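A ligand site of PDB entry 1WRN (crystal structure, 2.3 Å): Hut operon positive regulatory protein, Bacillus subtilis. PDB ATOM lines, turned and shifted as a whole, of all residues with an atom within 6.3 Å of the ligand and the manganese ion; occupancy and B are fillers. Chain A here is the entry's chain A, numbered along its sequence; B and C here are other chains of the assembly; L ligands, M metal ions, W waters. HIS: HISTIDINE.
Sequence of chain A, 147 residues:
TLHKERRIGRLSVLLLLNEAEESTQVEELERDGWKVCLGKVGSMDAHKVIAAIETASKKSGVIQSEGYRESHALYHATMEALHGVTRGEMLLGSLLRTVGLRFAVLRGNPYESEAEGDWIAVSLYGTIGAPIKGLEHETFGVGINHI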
ATOM      1  N   VAL A  85      23.526  15.625  -4.984  1.00  0.00           N
ATOM      2  CA  VAL A  85      23.489  14.398  -4.221  1.00  0.00           C
ATOM      3  C   VAL A  85      24.175  13.267  -4.967  1.00  0.00           C
ATOM      4  O   VAL A  85      24.980  12.555  -4.387  1.00  0.00           O
ATOM      5  CB  VAL A  85      22.052  13.974  -3.874  1.00  0.00           C
ATOM      6  CG1 VAL A  85      22.048  12.520  -3.391  1.00  0.00           C
ATOM      7  CG2 VAL A  85      21.479  14.892  -2.788  1.00  0.00           C
ATOM      8  N   THR A  86      23.854  13.141  -6.260  1.00  0.00           N
ATOM      9  CA  THR A  86      24.430  12.059  -7.074  1.00  0.00           C
ATOM     10  C   THR A  86      25.765  12.382  -7.740  1.00  0.00           C
ATOM     11  O   THR A  86      26.467  11.477  -8.178  1.00  0.00           O
ATOM     12  CB  THR A  86      23.429  11.577  -8.169  1.00  0.00           C
ATOM     13  OG1 THR A  86      23.183  12.612  -9.112  1.00  0.00           O
ATOM     14  CG2 THR A  86      22.104  11.157  -7.546  1.00  0.00           C
ATOM     15  N   ARG A  87      26.107  13.657  -7.827  1.00  0.00           N
ATOM     16  CA  ARG A  87      27.379  14.079  -8.425  1.00  0.00           C
ATOM     17  C   ARG A  87      27.837  13.358  -9.689  1.00  0.00           C
ATOM     18  O   ARG A  87      28.898  12.738  -9.682  1.00  0.00           O
ATOM     19  CB  ARG A  87      28.502  13.954  -7.385  1.00  0.00           C
ATOM     20  CG  ARG A  87      28.445  14.936  -6.244  1.00  0.00           C
ATOM     21  CD  ARG A  87      28.874  14.259  -4.965  1.00  0.00           C
ATOM     22  NE  ARG A  87      27.942  13.187  -4.621  1.00  0.00           N
ATOM     23  CZ  ARG A  87      28.277  11.918  -4.378  1.00  0.00           C
ATOM     24  NH1 ARG A  87      29.549  11.529  -4.437  1.00  0.00           N
ATOM     25  NH2 ARG A  87      27.341  11.029  -4.072  1.00  0.00           N
ATOM     26  N   LEU A  95      23.291   1.605  -9.289  1.00  0.00           N
ATOM     27  CA  LEU A  95      24.733   1.823  -9.169  1.00  0.00           C
ATOM     28  C   LEU A  95      25.111   1.383  -7.770  1.00  0.00           C
ATOM     29  O   LEU A  95      26.025   1.922  -7.141  1.00  0.00           O
ATOM     30  CB  LEU A  95      25.091   3.297  -9.365  1.00  0.00           C
ATOM     31  CG  LEU A  95      24.994   3.866 -10.787  1.00  0.00           C
ATOM     32  CD1 LEU A  95      25.528   5.290 -10.774  1.00  0.00           C
ATOM     33  CD2 LEU A  95      25.796   3.008 -11.762  1.00  0.00           C
ATOM     34  N   LEU A  96      24.365   0.390  -7.307  1.00  0.00           N
ATOM     35  CA  LEU A  96      24.532  -0.208  -5.996  1.00  0.00           C
ATOM     36  C   LEU A  96      24.707   0.784  -4.853  1.00  0.00           C
ATOM     37  O   LEU A  96      25.588   0.630  -4.017  1.00  0.00           O
ATOM     38  CB  LEU A  96      25.713  -1.178  -6.016  1.00  0.00           C
ATOM     39  CG  LEU A  96      25.656  -2.255  -4.925  1.00  0.00           C
ATOM     40  CD1 LEU A  96      24.292  -2.936  -4.940  1.00  0.00           C
ATOM     41  CD2 LEU A  96      26.763  -3.278  -5.151  1.00  0.00           C
ATOM     42  N   ARG A  97      23.861   1.809  -4.795  1.00  0.00           N
ATOM     43  CA  ARG A  97      23.953   2.763  -3.701  1.00  0.00           C
ATOM     44  C   ARG A  97      22.582   3.240  -3.296  1.00  0.00           C
ATOM     45  O   ARG A  97      21.621   3.165  -4.061  1.00  0.00           O
ATOM     46  CB  ARG A  97      24.838   3.973  -4.067  1.00  0.00           C
ATOM     47  CG  ARG A  97      24.320   4.864  -5.166  1.00  0.00           C
ATOM     48  CD  ARG A  97      25.225   6.082  -5.282  1.00  0.00           C
ATOM     49  NE  ARG A  97      24.954   6.830  -6.496  1.00  0.00           N
ATOM     50  CZ  ARG A  97      25.713   7.812  -6.964  1.00  0.00           C
ATOM     51  NH1 ARG A  97      26.810   8.196  -6.309  1.00  0.00           N
ATOM     52  NH2 ARG A  97      25.397   8.411  -8.095  1.00  0.00           N
ATOM     53  N   THR A  98      22.475   3.735  -2.076  1.00  0.00           N
ATOM     54  CA  THR A  98      21.202   4.210  -1.570  1.00  0.00           C
ATOM     55  C   THR A  98      21.382   5.492  -0.766  1.00  0.00           C
ATOM     56  O   THR A  98      22.497   5.818  -0.336  1.00  0.00           O
ATOM     57  CB  THR A  98      20.527   3.099  -0.716  1.00  0.00           C
ATOM     58  OG1 THR A  98      19.321   3.589  -0.132  1.00  0.00           O
ATOM     59  CG2 THR A  98      21.462   2.629   0.378  1.00  0.00           C
ATOM     60  N   ILE A 128      24.673   8.775   1.691  1.00  0.00           N
ATOM     61  CA  ILE A 128      24.664   8.043   0.441  1.00  0.00           C
ATOM     62  C   ILE A 128      25.762   6.995   0.644  1.00  0.00           C
ATOM     63  O   ILE A 128      26.804   7.306   1.214  1.00  0.00           O
ATOM     64  CB  ILE A 128      24.998   8.929  -0.784  1.00  0.00           C
ATOM     65  CG1 ILE A 128      24.897   8.098  -2.067  1.00  0.00           C
ATOM     66  CG2 ILE A 128      26.405   9.533  -0.664  1.00  0.00           C
ATOM     67  CD1 ILE A 128      24.972   8.911  -3.346  1.00  0.00           C
ATOM     68  N   GLY A 129      25.497   5.771   0.211  1.00  0.00           N
ATOM     69  CA  GLY A 129      26.468   4.703   0.374  1.00  0.00           C
ATOM     70  C   GLY A 129      25.888   3.360   0.000  1.00  0.00           C
ATOM     71  O   GLY A 129      24.800   3.281  -0.558  1.00  0.00           O
ATOM     72  N   ALA A 130      26.618   2.299   0.319  1.00  0.00           N
ATOM     73  CA  ALA A 130      26.182   0.941   0.002  1.00  0.00           C
ATOM     74  C   ALA A 130      24.893   0.535   0.711  1.00  0.00           C
ATOM     75  O   ALA A 130      24.511   1.119   1.727  1.00  0.00           O
ATOM     76  CB  ALA A 130      27.294  -0.049   0.346  1.00  0.00           C
ATOM     77  N   PRO A 131      24.193  -0.476   0.164  1.00  0.00           N
ATOM     78  CA  PRO A 131      22.936  -0.977   0.754  1.00  0.00           C
ATOM     79  C   PRO A 131      23.119  -1.367   2.217  1.00  0.00           C
ATOM     80  O   PRO A 131      22.166  -1.417   2.983  1.00  0.00           O
ATOM     81  CB  PRO A 131      22.600  -2.178  -0.128  1.00  0.00           C
ATOM     82  CG  PRO A 131      23.107  -1.733  -1.477  1.00  0.00           C
ATOM     83  CD  PRO A 131      24.441  -1.110  -1.143  1.00  0.00           C
ATOM     84  N   LEU A 135      28.396   1.599   5.758  1.00  0.00           N
ATOM     85  CA  LEU A 135      29.234   2.029   4.654  1.00  0.00           C
ATOM     86  C   LEU A 135      28.632   3.190   3.854  1.00  0.00           C
ATOM     87  O   LEU A 135      27.981   2.989   2.841  1.00  0.00           O
ATOM     88  CB  LEU A 135      29.488   0.837   3.729  1.00  0.00           C
ATOM     89  CG  LEU A 135      29.880  -0.442   4.479  1.00  0.00           C
ATOM     90  CD1 LEU A 135      30.277  -1.516   3.486  1.00  0.00           C
ATOM     91  CD2 LEU A 135      31.033  -0.134   5.428  1.00  0.00           C
ATOM     92  N   GLU A 136      28.874   4.423   4.314  1.00  0.00           N
ATOM     93  CA  GLU A 136      28.333   5.575   3.614  1.00  0.00           C
ATOM     94  C   GLU A 136      28.969   6.865   4.139  1.00  0.00           C
ATOM     95  O   GLU A 136      29.671   6.862   5.150  1.00  0.00           O
ATOM     96  CB  GLU A 136      26.824   5.643   3.820  1.00  0.00           C
ATOM     97  CG  GLU A 136      26.428   6.186   5.183  1.00  0.00           C
ATOM     98  CD  GLU A 136      25.458   5.294   5.927  1.00  0.00           C
ATOM     99  OE1 GLU A 136      25.014   4.281   5.345  1.00  0.00           O
ATOM    100  OE2 GLU A 136      25.142   5.622   7.086  1.00  0.00           O
ATOM    101  N   HIS A 137      28.713   7.964   3.431  1.00  0.00           N
ATOM    102  CA  HIS A 137      29.217   9.274   3.832  1.00  0.00           C
ATOM    103  C   HIS A 137      28.128  10.300   3.508  1.00  0.00           C
ATOM    104  O   HIS A 137      27.131   9.978   2.849  1.00  0.00           O
ATOM    105  CB  HIS A 137      30.537   9.622   3.131  1.00  0.00           C
ATOM    106  CG  HIS A 137      30.447   9.703   1.641  1.00  0.00           C
ATOM    107  ND1 HIS A 137      29.628  10.602   0.987  1.00  0.00           N
ATOM    108  CD2 HIS A 137      31.128   9.049   0.671  1.00  0.00           C
ATOM    109  CE1 HIS A 137      29.814  10.494  -0.320  1.00  0.00           C
ATOM    110  NE2 HIS A 137      30.718   9.563  -0.533  1.00  0.00           N
ATOM    111  N   GLU B  54      33.399  -5.949  -6.125  1.00  0.00           N
ATOM    112  CA  GLU B  54      33.586  -5.730  -4.702  1.00  0.00           C
ATOM    113  C   GLU B  54      33.717  -7.077  -3.997  1.00  0.00           C
ATOM    114  O   GLU B  54      34.631  -7.291  -3.208  1.00  0.00           O
ATOM    115  CB  GLU B  54      32.397  -4.973  -4.103  1.00  0.00           C
ATOM    116  CG  GLU B  54      32.570  -4.644  -2.631  1.00  0.00           C
ATOM    117  CD  GLU B  54      31.354  -3.956  -2.027  1.00  0.00           C
ATOM    118  OE1 GLU B  54      30.364  -3.727  -2.755  1.00  0.00           O
ATOM    119  OE2 GLU B  54      31.384  -3.633  -0.823  1.00  0.00           O
ATOM    120  N   TYR B  68      34.810   1.104   5.957  1.00  0.00           N
ATOM    121  CA  TYR B  68      34.268   1.765   4.782  1.00  0.00           C
ATOM    122  C   TYR B  68      35.331   2.321   3.836  1.00  0.00           C
ATOM    123  O   TYR B  68      35.178   2.262   2.621  1.00  0.00           O
ATOM    124  CB  TYR B  68      33.348   2.896   5.214  1.00  0.00           C
ATOM    125  CG  TYR B  68      32.670   3.574   4.058  1.00  0.00           C
ATOM    126  CD1 TYR B  68      32.287   2.855   2.934  1.00  0.00           C
ATOM    127  CD2 TYR B  68      32.358   4.939   4.106  1.00  0.00           C
ATOM    128  CE1 TYR B  68      31.621   3.455   1.892  1.00  0.00           C
ATOM    129  CE2 TYR B  68      31.702   5.540   3.065  1.00  0.00           C
ATOM    130  CZ  TYR B  68      31.323   4.799   1.962  1.00  0.00           C
ATOM    131  OH  TYR B  68      30.620   5.377   0.937  1.00  0.00           O
ATOM    132  N   SER B  71      36.347   0.265   0.744  1.00  0.00           N
ATOM    133  CA  SER B  71      35.191   0.059  -0.107  1.00  0.00           C
ATOM    134  C   SER B  71      34.917   1.366  -0.866  1.00  0.00           C
ATOM    135  O   SER B  71      34.530   1.345  -2.027  1.00  0.00           O
ATOM    136  CB  SER B  71      33.986  -0.331   0.748  1.00  0.00           C
ATOM    137  OG  SER B  71      34.125  -1.672   1.176  1.00  0.00           O
ATOM    138  N   HIS B  72      35.154   2.486  -0.214  1.00  0.00           N
ATOM    139  CA  HIS B  72      34.950   3.781  -0.860  1.00  0.00           C
ATOM    140  C   HIS B  72      35.967   3.928  -1.993  1.00  0.00           C
ATOM    141  O   HIS B  72      35.606   4.286  -3.121  1.00  0.00           O
ATOM    142  CB  HIS B  72      35.124   4.904   0.158  1.00  0.00           C
ATOM    143  CG  HIS B  72      34.713   6.244  -0.357  1.00  0.00           C
ATOM    144  ND1 HIS B  72      35.623   7.217  -0.714  1.00  0.00           N
ATOM    145  CD2 HIS B  72      33.486   6.766  -0.605  1.00  0.00           C
ATOM    146  CE1 HIS B  72      34.970   8.274  -1.165  1.00  0.00           C
ATOM    147  NE2 HIS B  72      33.673   8.020  -1.109  1.00  0.00           N
ATOM    148  N   TYR B  75      34.921   1.483  -4.873  1.00  0.00           N
ATOM    149  CA  TYR B  75      33.675   1.854  -5.507  1.00  0.00           C
ATOM    150  C   TYR B  75      33.906   2.969  -6.516  1.00  0.00           C
ATOM    151  O   TYR B  75      33.474   2.866  -7.668  1.00  0.00           O
ATOM    152  CB  TYR B  75      32.653   2.315  -4.459  1.00  0.00           C
ATOM    153  CG  TYR B  75      31.350   2.766  -5.070  1.00  0.00           C
ATOM    154  CD1 TYR B  75      31.195   4.047  -5.572  1.00  0.00           C
ATOM    155  CD2 TYR B  75      30.272   1.884  -5.170  1.00  0.00           C
ATOM    156  CE1 TYR B  75      30.011   4.456  -6.173  1.00  0.00           C
ATOM    157  CE2 TYR B  75      29.081   2.283  -5.767  1.00  0.00           C
ATOM    158  CZ  TYR B  75      28.955   3.570  -6.268  1.00  0.00           C
ATOM    159  OH  TYR B  75      27.773   3.970  -6.842  1.00  0.00           O
ATOM    160  N   HIS B  76      34.603   4.014  -6.084  1.00  0.00           N
ATOM    161  CA  HIS B  76      34.861   5.130  -6.980  1.00  0.00           C
ATOM    162  C   HIS B  76      35.748   4.752  -8.159  1.00  0.00           C
ATOM    163  O   HIS B  76      35.603   5.305  -9.238  1.00  0.00           O
ATOM    164  CB  HIS B  76      35.433   6.335  -6.182  1.00  0.00           C
ATOM    165  CG  HIS B  76      34.387   7.121  -5.436  1.00  0.00           C
ATOM    166  ND1 HIS B  76      33.564   8.036  -6.053  1.00  0.00           N
ATOM    167  CD2 HIS B  76      33.981   7.057  -4.145  1.00  0.00           C
ATOM    168  CE1 HIS B  76      32.699   8.502  -5.175  1.00  0.00           C
ATOM    169  NE2 HIS B  76      32.928   7.925  -4.009  1.00  0.00           N
ATOM    170  N   GLU C  80      33.614  16.910  -6.910  1.00  0.00           N
ATOM    171  CA  GLU C  80      32.289  16.527  -6.469  1.00  0.00           C
ATOM    172  C   GLU C  80      31.485  17.668  -5.918  1.00  0.00           C
ATOM    173  O   GLU C  80      30.274  17.668  -5.998  1.00  0.00           O
ATOM    174  CB  GLU C  80      32.354  15.363  -5.468  1.00  0.00           C
ATOM    175  CG  GLU C  80      32.800  14.041  -6.147  1.00  0.00           C
ATOM    176  CD  GLU C  80      32.662  12.840  -5.264  1.00  0.00           C
ATOM    177  OE1 GLU C  80      31.891  12.915  -4.278  1.00  0.00           O
ATOM    178  N   TRP C 119      39.400  11.921   6.432  1.00  0.00           N
ATOM    179  CA  TRP C 119      38.518  12.184   5.305  1.00  0.00           C
ATOM    180  C   TRP C 119      38.546  13.685   5.058  1.00  0.00           C
ATOM    181  O   TRP C 119      38.978  14.455   5.912  1.00  0.00           O
ATOM    182  CB  TRP C 119      37.092  11.709   5.610  1.00  0.00           C
ATOM    183  CG  TRP C 119      36.952  10.198   5.617  1.00  0.00           C
ATOM    184  CD1 TRP C 119      37.482   9.325   6.533  1.00  0.00           C
ATOM    185  CD2 TRP C 119      36.306   9.395   4.631  1.00  0.00           C
ATOM    186  NE1 TRP C 119      37.199   8.031   6.173  1.00  0.00           N
ATOM    187  CE2 TRP C 119      36.481   8.036   5.005  1.00  0.00           C
ATOM    188  CE3 TRP C 119      35.594   9.680   3.460  1.00  0.00           C
ATOM    189  CZ2 TRP C 119      35.970   6.974   4.250  1.00  0.00           C
ATOM    190  CZ3 TRP C 119      35.084   8.618   2.705  1.00  0.00           C
ATOM    191  CH2 TRP C 119      35.283   7.285   3.103  1.00  0.00           C
ATOM    192  N   ILE C 144      32.782  15.029  -0.586  1.00  0.00           N
ATOM    193  CA  ILE C 144      33.448  14.318   0.505  1.00  0.00           C
ATOM    194  C   ILE C 144      34.320  13.195  -0.057  1.00  0.00           C
ATOM    195  O   ILE C 144      33.943  12.522  -0.992  1.00  0.00           O
ATOM    196  CB  ILE C 144      32.405  13.754   1.523  1.00  0.00           C
ATOM    197  CG1 ILE C 144      31.784  14.914   2.308  1.00  0.00           C
ATOM    198  CG2 ILE C 144      33.069  12.764   2.497  1.00  0.00           C
ATOM    199  CD1 ILE C 144      30.735  14.482   3.300  1.00  0.00           C
ATOM    200  N   ASN C 145      35.512  13.007   0.512  1.00  0.00           N
ATOM    201  CA  ASN C 145      36.403  11.988  -0.006  1.00  0.00           C
ATOM    202  C   ASN C 145      37.344  11.482   1.082  1.00  0.00           C
ATOM    203  O   ASN C 145      37.593  12.184   2.055  1.00  0.00           O
ATOM    204  CB  ASN C 145      37.220  12.584  -1.154  1.00  0.00           C
ATOM    205  CG  ASN C 145      37.990  11.544  -1.930  1.00  0.00           C
ATOM    206  OD1 ASN C 145      37.714  10.346  -1.848  1.00  0.00           O
ATOM    207  ND2 ASN C 145      38.965  12.005  -2.713  1.00  0.00           N
HETATM  208  CA  HIS L   1      29.588   6.678  -2.863  1.00  0.00           C
HETATM  209  C   HIS L   1      29.116   7.987  -3.493  1.00  0.00           C
HETATM  210  O   HIS L   1      29.866   8.982  -3.428  1.00  0.00           O
HETATM  211  CB  HIS L   1      28.370   5.850  -2.387  1.00  0.00           C
HETATM  212  CG  HIS L   1      28.660   4.400  -2.179  1.00  0.00           C
HETATM  213  ND1 HIS L   1      29.480   3.951  -1.164  1.00  0.00           N
HETATM  214  CD2 HIS L   1      28.287   3.300  -2.879  1.00  0.00           C
HETATM  215  CE1 HIS L   1      29.599   2.641  -1.259  1.00  0.00           C
HETATM  216  NE2 HIS L   1      28.890   2.214  -2.278  1.00  0.00           N
HETATM  217  OXT HIS L   1      28.005   8.022  -4.061  1.00  0.00           O
HETATM  218 MN    MN M   1      31.791   8.696  -2.254  1.00  0.00          MN
HETATM  219  O   HOH W   1      32.886  10.606  -2.665  1.00  0.00           O
HETATM  220  O   HOH W   2      27.710  -0.163  -3.001  1.00  0.00           O
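Residues that only touch the ligand: Tyr 75 of chain B (3.2 Å), Ile 128 (3.2 Å), Gly 129 (3.4 Å) and Leu 96 (3.96 Å).
Of the 24 residues printed, 10 come within 4 Å of the ligand.
The nearest printed residue that does not touch the ligand is Leu 135 (4.4 Å).
The backbone carbonyl oxygen of Gly 129 is in hydrogen-bond range of the backbone NH of Thr 98, 2.8 Å away.
The guanidinium group (NH1) of Arg 87 is in salt-bridge range of the side-chain carboxylate (OE1) of Glu 80 of chain C (2.7 Å).
NH2 of Arg 97 is in hydrogen-bond range of O of Thr 86, 3.2 Å away.
The side-chain hydroxyl (OH) of Tyr 75 of chain B sits at hydrogen-bond distance from the backbone carbonyl oxygen (O) of Leu 95 (2.7 Å).
The backbone carbonyl oxygen (O) of Leu 135 is in hydrogen-bond range of the backbone NH (N) of Ala 130 (2.9 Å).
The guanidinium group of Arg 87 lies within hydrogen-bond range of the backbone carbonyl oxygen of Val 85 (2.8 Å).
O of His 137 lies within hydrogen-bond range of N of Ile 128 (3.0 Å).
Water W1 lies within hydrogen-bond range of O of Ile 144 of chain C and OE1 of Glu 80 of chain C.
Water W2 lies within hydrogen-bond range of O of Leu 96 (2.5 Å) and NE2 of the ligand (2.8 Å).
N of Ala 130 lies close to NE2 of the ligand (3.5 Å).
NH1 of Arg 97 is in salt-bridge range of OXT of the ligand (2.6 Å).
An oxygen (OXT) of the ligand is in salt-bridge range of the guanidinium group (NH2) of Arg 87 (3.1 Å).
The side-chain hydroxyl of Tyr 68 of chain B lies within hydrogen-bond range of a nitrogen (ND1) of the ligand, 2.8 Å away.
The manganese ion is bound by a ring nitrogen (NE2) of His 137 (2.2 Å), a ring nitrogen (NE2) of His 76 of chain B (2.2 Å), water W1 (2.2 Å), an oxygen (O) of the ligand (2.3 Å) and a ring nitrogen (NE2) of His 72 of chain B (2.3 Å).
The manganese ion has five donor atoms within binding distance.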
